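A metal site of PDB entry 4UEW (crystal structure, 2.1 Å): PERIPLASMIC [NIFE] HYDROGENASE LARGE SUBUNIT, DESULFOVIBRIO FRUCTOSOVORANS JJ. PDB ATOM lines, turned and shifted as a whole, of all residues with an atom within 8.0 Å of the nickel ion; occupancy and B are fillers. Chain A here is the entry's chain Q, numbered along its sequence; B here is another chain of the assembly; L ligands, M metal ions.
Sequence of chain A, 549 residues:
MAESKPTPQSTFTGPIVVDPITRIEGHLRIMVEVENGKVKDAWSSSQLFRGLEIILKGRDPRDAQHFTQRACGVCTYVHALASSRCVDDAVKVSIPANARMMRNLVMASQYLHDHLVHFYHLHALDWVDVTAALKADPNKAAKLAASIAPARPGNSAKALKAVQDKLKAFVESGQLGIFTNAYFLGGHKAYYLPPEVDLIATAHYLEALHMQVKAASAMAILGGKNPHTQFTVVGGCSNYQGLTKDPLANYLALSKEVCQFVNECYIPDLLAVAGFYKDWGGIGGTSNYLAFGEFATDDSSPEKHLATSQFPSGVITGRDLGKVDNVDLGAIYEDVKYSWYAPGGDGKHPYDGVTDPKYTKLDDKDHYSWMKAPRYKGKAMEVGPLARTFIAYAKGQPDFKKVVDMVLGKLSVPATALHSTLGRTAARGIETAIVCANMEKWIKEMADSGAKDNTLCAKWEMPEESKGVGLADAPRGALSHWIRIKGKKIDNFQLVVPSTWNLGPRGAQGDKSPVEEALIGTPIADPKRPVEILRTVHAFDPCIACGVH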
ATOM      1  N   GLU A  25     -11.859  14.261  15.306  1.00  0.00           N
ATOM      2  CA  GLU A  25     -12.101  15.544  15.927  1.00  0.00           C
ATOM      3  C   GLU A  25     -13.472  15.437  16.622  1.00  0.00           C
ATOM      4  O   GLU A  25     -14.479  14.983  16.024  1.00  0.00           O
ATOM      5  CB  GLU A  25     -12.102  16.654  14.868  1.00  0.00           C
ATOM      6  CG  GLU A  25     -12.018  18.068  15.440  1.00  0.00           C
ATOM      7  CD  GLU A  25     -13.229  18.392  16.308  1.00  0.00           C
ATOM      8  OE1 GLU A  25     -14.365  18.122  15.827  1.00  0.00           O
ATOM      9  OE2 GLU A  25     -13.063  18.894  17.453  1.00  0.00           O
ATOM     10  N   GLN A  69     -15.133  29.988  11.492  1.00  0.00           N
ATOM     11  CA  GLN A  69     -13.899  29.229  11.331  1.00  0.00           C
ATOM     12  C   GLN A  69     -13.666  28.374  12.577  1.00  0.00           C
ATOM     13  O   GLN A  69     -13.190  27.262  12.487  1.00  0.00           O
ATOM     14  CB  GLN A  69     -12.696  30.126  11.021  1.00  0.00           C
ATOM     15  CG  GLN A  69     -11.515  29.278  10.503  1.00  0.00           C
ATOM     16  CD  GLN A  69     -10.281  30.068  10.112  1.00  0.00           C
ATOM     17  OE1 GLN A  69      -9.318  29.506   9.599  1.00  0.00           O
ATOM     18  NE2 GLN A  69     -10.292  31.352  10.352  1.00  0.00           N
ATOM     19  N   ALA A  71     -15.722  26.703  14.117  1.00  0.00           N
ATOM     20  CA  ALA A  71     -16.418  25.416  14.092  1.00  0.00           C
ATOM     21  C   ALA A  71     -15.444  24.249  14.135  1.00  0.00           C
ATOM     22  O   ALA A  71     -15.825  23.155  14.604  1.00  0.00           O
ATOM     23  CB  ALA A  71     -17.321  25.289  12.875  1.00  0.00           C
ATOM     24  N   CYS A  72     -14.206  24.451  13.643  1.00  0.00           N
ATOM     25  CA  CYS A  72     -13.206  23.393  13.545  1.00  0.00           C
ATOM     26  C   CYS A  72     -11.788  23.905  13.327  1.00  0.00           C
ATOM     27  O   CYS A  72     -11.540  24.709  12.430  1.00  0.00           O
ATOM     28  CB  CYS A  72     -13.563  22.436  12.410  1.00  0.00           C
ATOM     29  SG  CYS A  72     -12.586  20.899  12.497  1.00  0.00           S
ATOM     30  N   GLY A  73     -10.829  23.378  14.104  1.00  0.00           N
ATOM     31  CA  GLY A  73      -9.423  23.720  13.955  1.00  0.00           C
ATOM     32  C   GLY A  73      -8.624  22.659  13.228  1.00  0.00           C
ATOM     33  O   GLY A  73      -7.405  22.832  13.011  1.00  0.00           O
ATOM     34  N   VAL A  74      -9.282  21.551  12.880  1.00  0.00           N
ATOM     35  CA  VAL A  74      -8.713  20.499  12.082  1.00  0.00           C
ATOM     36  C   VAL A  74      -8.945  20.862  10.619  1.00  0.00           C
ATOM     37  O   VAL A  74      -7.980  21.107   9.879  1.00  0.00           O
ATOM     38  CB  VAL A  74      -9.268  19.099  12.436  1.00  0.00           C
ATOM     39  CG1 VAL A  74      -8.716  18.083  11.441  1.00  0.00           C
ATOM     40  CG2 VAL A  74      -8.903  18.740  13.877  1.00  0.00           C
ATOM     41  N   CYS A  75     -10.233  20.951  10.223  1.00  0.00           N
ATOM     42  CA  CYS A  75     -10.548  21.628   8.944  1.00  0.00           C
ATOM     43  C   CYS A  75     -10.529  23.133   9.175  1.00  0.00           C
ATOM     44  O   CYS A  75     -11.524  23.832   8.941  1.00  0.00           O
ATOM     45  CB  CYS A  75     -11.872  21.144   8.307  1.00  0.00           C
ATOM     46  SG  CYS A  75     -13.372  21.320   9.332  1.00  0.00           S
ATOM     47  N   THR A  76      -9.377  23.650   9.614  1.00  0.00           N
ATOM     48  CA  THR A  76      -9.229  25.080   9.773  1.00  0.00           C
ATOM     49  C   THR A  76      -9.425  25.677   8.372  1.00  0.00           C
ATOM     50  O   THR A  76      -9.402  24.931   7.370  1.00  0.00           O
ATOM     51  CB  THR A  76      -7.869  25.471  10.424  1.00  0.00           C
ATOM     52  OG1 THR A  76      -7.895  26.858  10.750  1.00  0.00           O
ATOM     53  CG2 THR A  76      -6.649  25.194   9.521  1.00  0.00           C
ATOM     54  N   VAL A  78     -11.590  26.228   6.168  1.00  0.00           N
ATOM     55  CA  VAL A  78     -12.715  25.940   5.281  1.00  0.00           C
ATOM     56  C   VAL A  78     -14.020  26.701   5.592  1.00  0.00           C
ATOM     57  O   VAL A  78     -14.717  27.113   4.640  1.00  0.00           O
ATOM     58  CB  VAL A  78     -12.994  24.398   5.098  1.00  0.00           C
ATOM     59  CG1 VAL A  78     -11.713  23.648   4.774  1.00  0.00           C
ATOM     60  CG2 VAL A  78     -13.714  23.802   6.317  1.00  0.00           C
ATOM     61  N   HIS A  79     -14.349  26.878   6.880  1.00  0.00           N
ATOM     62  CA  HIS A  79     -15.518  27.655   7.285  1.00  0.00           C
ATOM     63  C   HIS A  79     -15.379  29.167   7.059  1.00  0.00           C
ATOM     64  O   HIS A  79     -16.352  29.843   6.656  1.00  0.00           O
ATOM     65  CB  HIS A  79     -15.902  27.372   8.757  1.00  0.00           C
ATOM     66  CG  HIS A  79     -16.298  25.944   8.997  1.00  0.00           C
ATOM     67  ND1 HIS A  79     -17.516  25.441   8.582  1.00  0.00           N
ATOM     68  CD2 HIS A  79     -15.649  24.908   9.589  1.00  0.00           C
ATOM     69  CE1 HIS A  79     -17.595  24.163   8.916  1.00  0.00           C
ATOM     70  NE2 HIS A  79     -16.481  23.823   9.540  1.00  0.00           N
ATOM     71  N   GLN A 110      -4.819  22.949   2.475  1.00  0.00           N
ATOM     72  CA  GLN A 110      -5.576  22.337   3.603  1.00  0.00           C
ATOM     73  C   GLN A 110      -5.799  20.852   3.342  1.00  0.00           C
ATOM     74  O   GLN A 110      -5.582  20.033   4.248  1.00  0.00           O
ATOM     75  CB  GLN A 110      -6.915  23.061   3.835  1.00  0.00           C
ATOM     76  CG  GLN A 110      -7.815  22.529   4.963  1.00  0.00           C
ATOM     77  CD  GLN A 110      -7.103  22.321   6.298  1.00  0.00           C
ATOM     78  OE1 GLN A 110      -6.204  23.098   6.695  1.00  0.00           O
ATOM     79  NE2 GLN A 110      -7.530  21.306   7.034  1.00  0.00           N
ATOM     80  N   ASP A 114      -4.511  18.117   5.937  1.00  0.00           N
ATOM     81  CA  ASP A 114      -5.592  17.339   6.602  1.00  0.00           C
ATOM     82  C   ASP A 114      -5.461  15.846   6.274  1.00  0.00           C
ATOM     83  O   ASP A 114      -5.410  15.008   7.165  1.00  0.00           O
ATOM     84  CB  ASP A 114      -6.969  17.892   6.169  1.00  0.00           C
ATOM     85  CG  ASP A 114      -8.101  17.683   7.234  1.00  0.00           C
ATOM     86  OD1 ASP A 114      -8.109  16.689   8.013  1.00  0.00           O
ATOM     87  OD2 ASP A 114      -8.996  18.558   7.310  1.00  0.00           O
ATOM     88  N   ALA A 474     -14.867  20.781   1.302  1.00  0.00           N
ATOM     89  CA  ALA A 474     -13.827  20.694   2.316  1.00  0.00           C
ATOM     90  C   ALA A 474     -13.207  19.295   2.285  1.00  0.00           C
ATOM     91  O   ALA A 474     -13.707  18.408   1.579  1.00  0.00           O
ATOM     92  CB  ALA A 474     -14.406  21.034   3.677  1.00  0.00           C
ATOM     93  N   PRO A 475     -12.091  19.076   2.995  1.00  0.00           N
ATOM     94  CA  PRO A 475     -11.486  17.725   2.928  1.00  0.00           C
ATOM     95  C   PRO A 475     -12.476  16.594   3.270  1.00  0.00           C
ATOM     96  O   PRO A 475     -12.301  15.457   2.837  1.00  0.00           O
ATOM     97  CB  PRO A 475     -10.355  17.799   3.929  1.00  0.00           C
ATOM     98  CG  PRO A 475      -9.966  19.247   3.985  1.00  0.00           C
ATOM     99  CD  PRO A 475     -11.211  20.043   3.694  1.00  0.00           C
ATOM    100  N   ARG A 476     -13.493  16.883   4.086  1.00  0.00           N
ATOM    101  CA  ARG A 476     -14.516  15.890   4.460  1.00  0.00           C
ATOM    102  C   ARG A 476     -15.745  15.916   3.591  1.00  0.00           C
ATOM    103  O   ARG A 476     -16.602  15.006   3.695  1.00  0.00           O
ATOM    104  CB  ARG A 476     -14.900  16.021   5.934  1.00  0.00           C
ATOM    105  CG  ARG A 476     -13.894  15.384   6.876  1.00  0.00           C
ATOM    106  CD  ARG A 476     -13.803  16.105   8.209  1.00  0.00           C
ATOM    107  NE  ARG A 476     -12.565  15.711   8.890  1.00  0.00           N
ATOM    108  CZ  ARG A 476     -11.424  16.374   8.758  1.00  0.00           C
ATOM    109  NH1 ARG A 476     -11.401  17.485   8.039  1.00  0.00           N
ATOM    110  NH2 ARG A 476     -10.314  15.923   9.371  1.00  0.00           N
ATOM    111  N   VAL A 497     -22.707  20.913   7.157  1.00  0.00           N
ATOM    112  CA  VAL A 497     -21.291  20.638   7.139  1.00  0.00           C
ATOM    113  C   VAL A 497     -21.145  19.172   6.767  1.00  0.00           C
ATOM    114  O   VAL A 497     -22.037  18.411   7.077  1.00  0.00           O
ATOM    115  CB  VAL A 497     -20.669  20.959   8.513  1.00  0.00           C
ATOM    116  CG1 VAL A 497     -19.167  20.765   8.500  1.00  0.00           C
ATOM    117  CG2 VAL A 497     -20.987  22.414   8.914  1.00  0.00           C
ATOM    118  N   PRO A 498     -20.028  18.786   6.092  1.00  0.00           N
ATOM    119  CA  PRO A 498     -19.890  17.415   5.596  1.00  0.00           C
ATOM    120  C   PRO A 498     -20.133  16.340   6.651  1.00  0.00           C
ATOM    121  O   PRO A 498     -20.869  15.394   6.361  1.00  0.00           O
ATOM    122  CB  PRO A 498     -18.425  17.345   5.081  1.00  0.00           C
ATOM    123  CG  PRO A 498     -17.828  18.699   5.255  1.00  0.00           C
ATOM    124  CD  PRO A 498     -18.971  19.662   5.539  1.00  0.00           C
ATOM    125  N   SER A 499     -19.539  16.462   7.843  1.00  0.00           N
ATOM    126  CA  SER A 499     -19.807  15.420   8.880  1.00  0.00           C
ATOM    127  C   SER A 499     -21.288  15.384   9.366  1.00  0.00           C
ATOM    128  O   SER A 499     -21.711  14.415  10.004  1.00  0.00           O
ATOM    129  CB  SER A 499     -18.853  15.558  10.063  1.00  0.00           C
ATOM    130  OG  SER A 499     -17.546  15.201   9.678  1.00  0.00           O
ATOM    131  N   ASP A 541     -13.657   9.979   8.255  1.00  0.00           N
ATOM    132  CA  ASP A 541     -12.913  11.169   8.728  1.00  0.00           C
ATOM    133  C   ASP A 541     -13.844  12.074   9.560  1.00  0.00           C
ATOM    134  O   ASP A 541     -14.076  13.226   9.235  1.00  0.00           O
ATOM    135  CB  ASP A 541     -12.360  11.921   7.505  1.00  0.00           C
ATOM    136  CG  ASP A 541     -11.274  12.910   7.863  1.00  0.00           C
ATOM    137  OD1 ASP A 541     -10.966  13.049   9.049  1.00  0.00           O
ATOM    138  OD2 ASP A 541     -10.713  13.579   6.971  1.00  0.00           O
ATOM    139  N   PRO A 542     -14.432  11.525  10.650  1.00  0.00           N
ATOM    140  CA  PRO A 542     -15.459  12.300  11.391  1.00  0.00           C
ATOM    141  C   PRO A 542     -14.933  13.592  12.023  1.00  0.00           C
ATOM    142  O   PRO A 542     -13.833  13.595  12.557  1.00  0.00           O
ATOM    143  CB  PRO A 542     -15.900  11.335  12.508  1.00  0.00           C
ATOM    144  CG  PRO A 542     -15.501   9.991  12.031  1.00  0.00           C
ATOM    145  CD  PRO A 542     -14.203  10.197  11.250  1.00  0.00           C
ATOM    146  N   CSO A 543     -15.710  14.659  11.928  1.00  0.00           N
ATOM    147  CA  CSO A 543     -15.372  15.934  12.552  1.00  0.00           C
ATOM    148  CB  CSO A 543     -14.936  16.930  11.476  1.00  0.00           C
ATOM    149  SG  CSO A 543     -13.844  18.164  12.137  1.00  0.00           S
ATOM    150  C   CSO A 543     -16.629  16.379  13.285  1.00  0.00           C
ATOM    151  O   CSO A 543     -17.562  16.885  12.667  1.00  0.00           O
ATOM    152  OD  CSO A 543     -14.799  18.917  13.369  1.00  0.00           O
ATOM    153  N   ILE A 544     -16.696  16.168  14.592  1.00  0.00           N
ATOM    154  CA  ILE A 544     -17.984  16.360  15.329  1.00  0.00           C
ATOM    155  C   ILE A 544     -18.301  17.816  15.686  1.00  0.00           C
ATOM    156  O   ILE A 544     -19.484  18.237  15.746  1.00  0.00           O
ATOM    157  CB  ILE A 544     -18.055  15.459  16.599  1.00  0.00           C
ATOM    158  CG1 ILE A 544     -17.678  13.997  16.263  1.00  0.00           C
ATOM    159  CG2 ILE A 544     -19.446  15.551  17.233  1.00  0.00           C
ATOM    160  CD1 ILE A 544     -18.550  13.338  15.197  1.00  0.00           C
ATOM    161  N   ALA A 545     -17.244  18.618  15.892  1.00  0.00           N
ATOM    162  CA  ALA A 545     -17.424  20.058  16.097  1.00  0.00           C
ATOM    163  C   ALA A 545     -17.934  20.670  14.779  1.00  0.00           C
ATOM    164  O   ALA A 545     -18.783  21.554  14.813  1.00  0.00           O
ATOM    165  CB  ALA A 545     -16.109  20.723  16.562  1.00  0.00           C
ATOM    166  N   CYS A 546     -17.442  20.173  13.636  1.00  0.00           N
ATOM    167  CA  CYS A 546     -17.990  20.561  12.309  1.00  0.00           C
ATOM    168  C   CYS A 546     -19.469  20.143  12.217  1.00  0.00           C
ATOM    169  O   CYS A 546     -20.335  20.985  11.937  1.00  0.00           O
ATOM    170  CB  CYS A 546     -17.225  19.910  11.148  1.00  0.00           C
ATOM    171  SG  CYS A 546     -15.847  20.895  10.541  1.00  0.00           S
ATOM    172  N   GLY A 547     -19.746  18.865  12.468  1.00  0.00           N
ATOM    173  CA  GLY A 547     -21.103  18.324  12.271  1.00  0.00           C
ATOM    174  C   GLY A 547     -22.170  19.028  13.087  1.00  0.00           C
ATOM    175  O   GLY A 547     -23.286  19.247  12.596  1.00  0.00           O
ATOM    176  N   CYS B  17     -12.697  23.264  19.394  1.00  0.00           N
ATOM    177  CA  CYS B  17     -12.659  22.960  17.964  1.00  0.00           C
ATOM    178  C   CYS B  17     -11.474  22.102  17.567  1.00  0.00           C
ATOM    179  O   CYS B  17     -11.331  21.735  16.391  1.00  0.00           O
ATOM    180  CB  CYS B  17     -12.610  24.256  17.146  1.00  0.00           C
ATOM    181  SG  CYS B  17     -10.968  25.041  17.092  1.00  0.00           S
ATOM    182  N   THR B  18     -10.597  21.812  18.532  1.00  0.00           N
ATOM    183  CA  THR B  18      -9.382  20.990  18.324  1.00  0.00           C
ATOM    184  C   THR B  18      -8.259  21.753  17.611  1.00  0.00           C
ATOM    185  O   THR B  18      -7.210  21.174  17.307  1.00  0.00           O
ATOM    186  CB  THR B  18      -9.728  19.624  17.676  1.00  0.00           C
ATOM    187  OG1 THR B  18     -10.837  19.053  18.370  1.00  0.00           O
ATOM    188  CG2 THR B  18      -8.596  18.636  17.786  1.00  0.00           C
HETATM  189 FE1  LIG L   1     -14.983  20.044   8.673  1.00  0.00          FE
HETATM  190  C1  LIG L   1     -16.252  18.614   8.549  1.00  0.00           C
HETATM  191  N1  LIG L   1     -17.016  17.733   8.478  1.00  0.00           N
HETATM  192  C2  LIG L   1     -14.074  19.368   7.150  1.00  0.00           C
HETATM  193  N2  LIG L   1     -13.496  18.952   6.253  1.00  0.00           N
HETATM  194  C3  LIG L   1     -15.930  20.968   7.522  1.00  0.00           C
HETATM  195  O1  LIG L   1     -16.538  21.584   6.760  1.00  0.00           O
HETATM  196 NI    NI M   1     -13.571  19.829  10.862  1.00  0.00          NI
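The side-chain hydroxyl (OG) of Ser 499 sits at hydrogen-bond distance from a nitrogen (N1) of the ligand (2.9 Å). An iron atom (FE1) of the ligand is bound by the side-chain sulfur (SG) of Cys 75 (2.2 Å). The backbone NH of Ser 499 is in hydrogen-bond range of a nitrogen (N1) of the ligand, at 2.9 Å. SG of Cys 546 is bound to FE1 of the ligand (2.2 Å). A nitrogen (N2) of the ligand is in hydrogen-bond range of the guanidinium group (NH1) of Arg 476, 3.1 Å away. N of Arg 476 lies within hydrogen-bond range of N2 of the ligand, 3.0 Å away.
OG of Ser 499 is in hydrogen-bond range of N of CSO 543. The side-chain sulfur of Cys 546 sits close to a ring nitrogen (NE2) of His 79, 3.2 Å away. The side-chain sulfur (SG) of Cys 72 lies close to the backbone NH (N) of Val 74, at 3.4 Å. OD of CSO 543 is in hydrogen-bond range of the side-chain carboxylate (OE1) of Glu 25, 2.6 Å away.
Within 4 Å of the nickel ion: Cys 72, Cys 75, CSO 543 and Cys 546. The nearest printed residue that does not touch the nickel ion is Arg 476 (4.3 Å).
The nickel ion is bound by SG of CSO 543 (2.1 Å), the side-chain sulfur (SG) of Cys 75 (2.1 Å), the side-chain sulfur (SG) of Cys 72 (2.2 Å) and the side-chain sulfur (SG) of Cys 546 (2.5 Å). The nickel ion has four donor atoms within binding distance.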
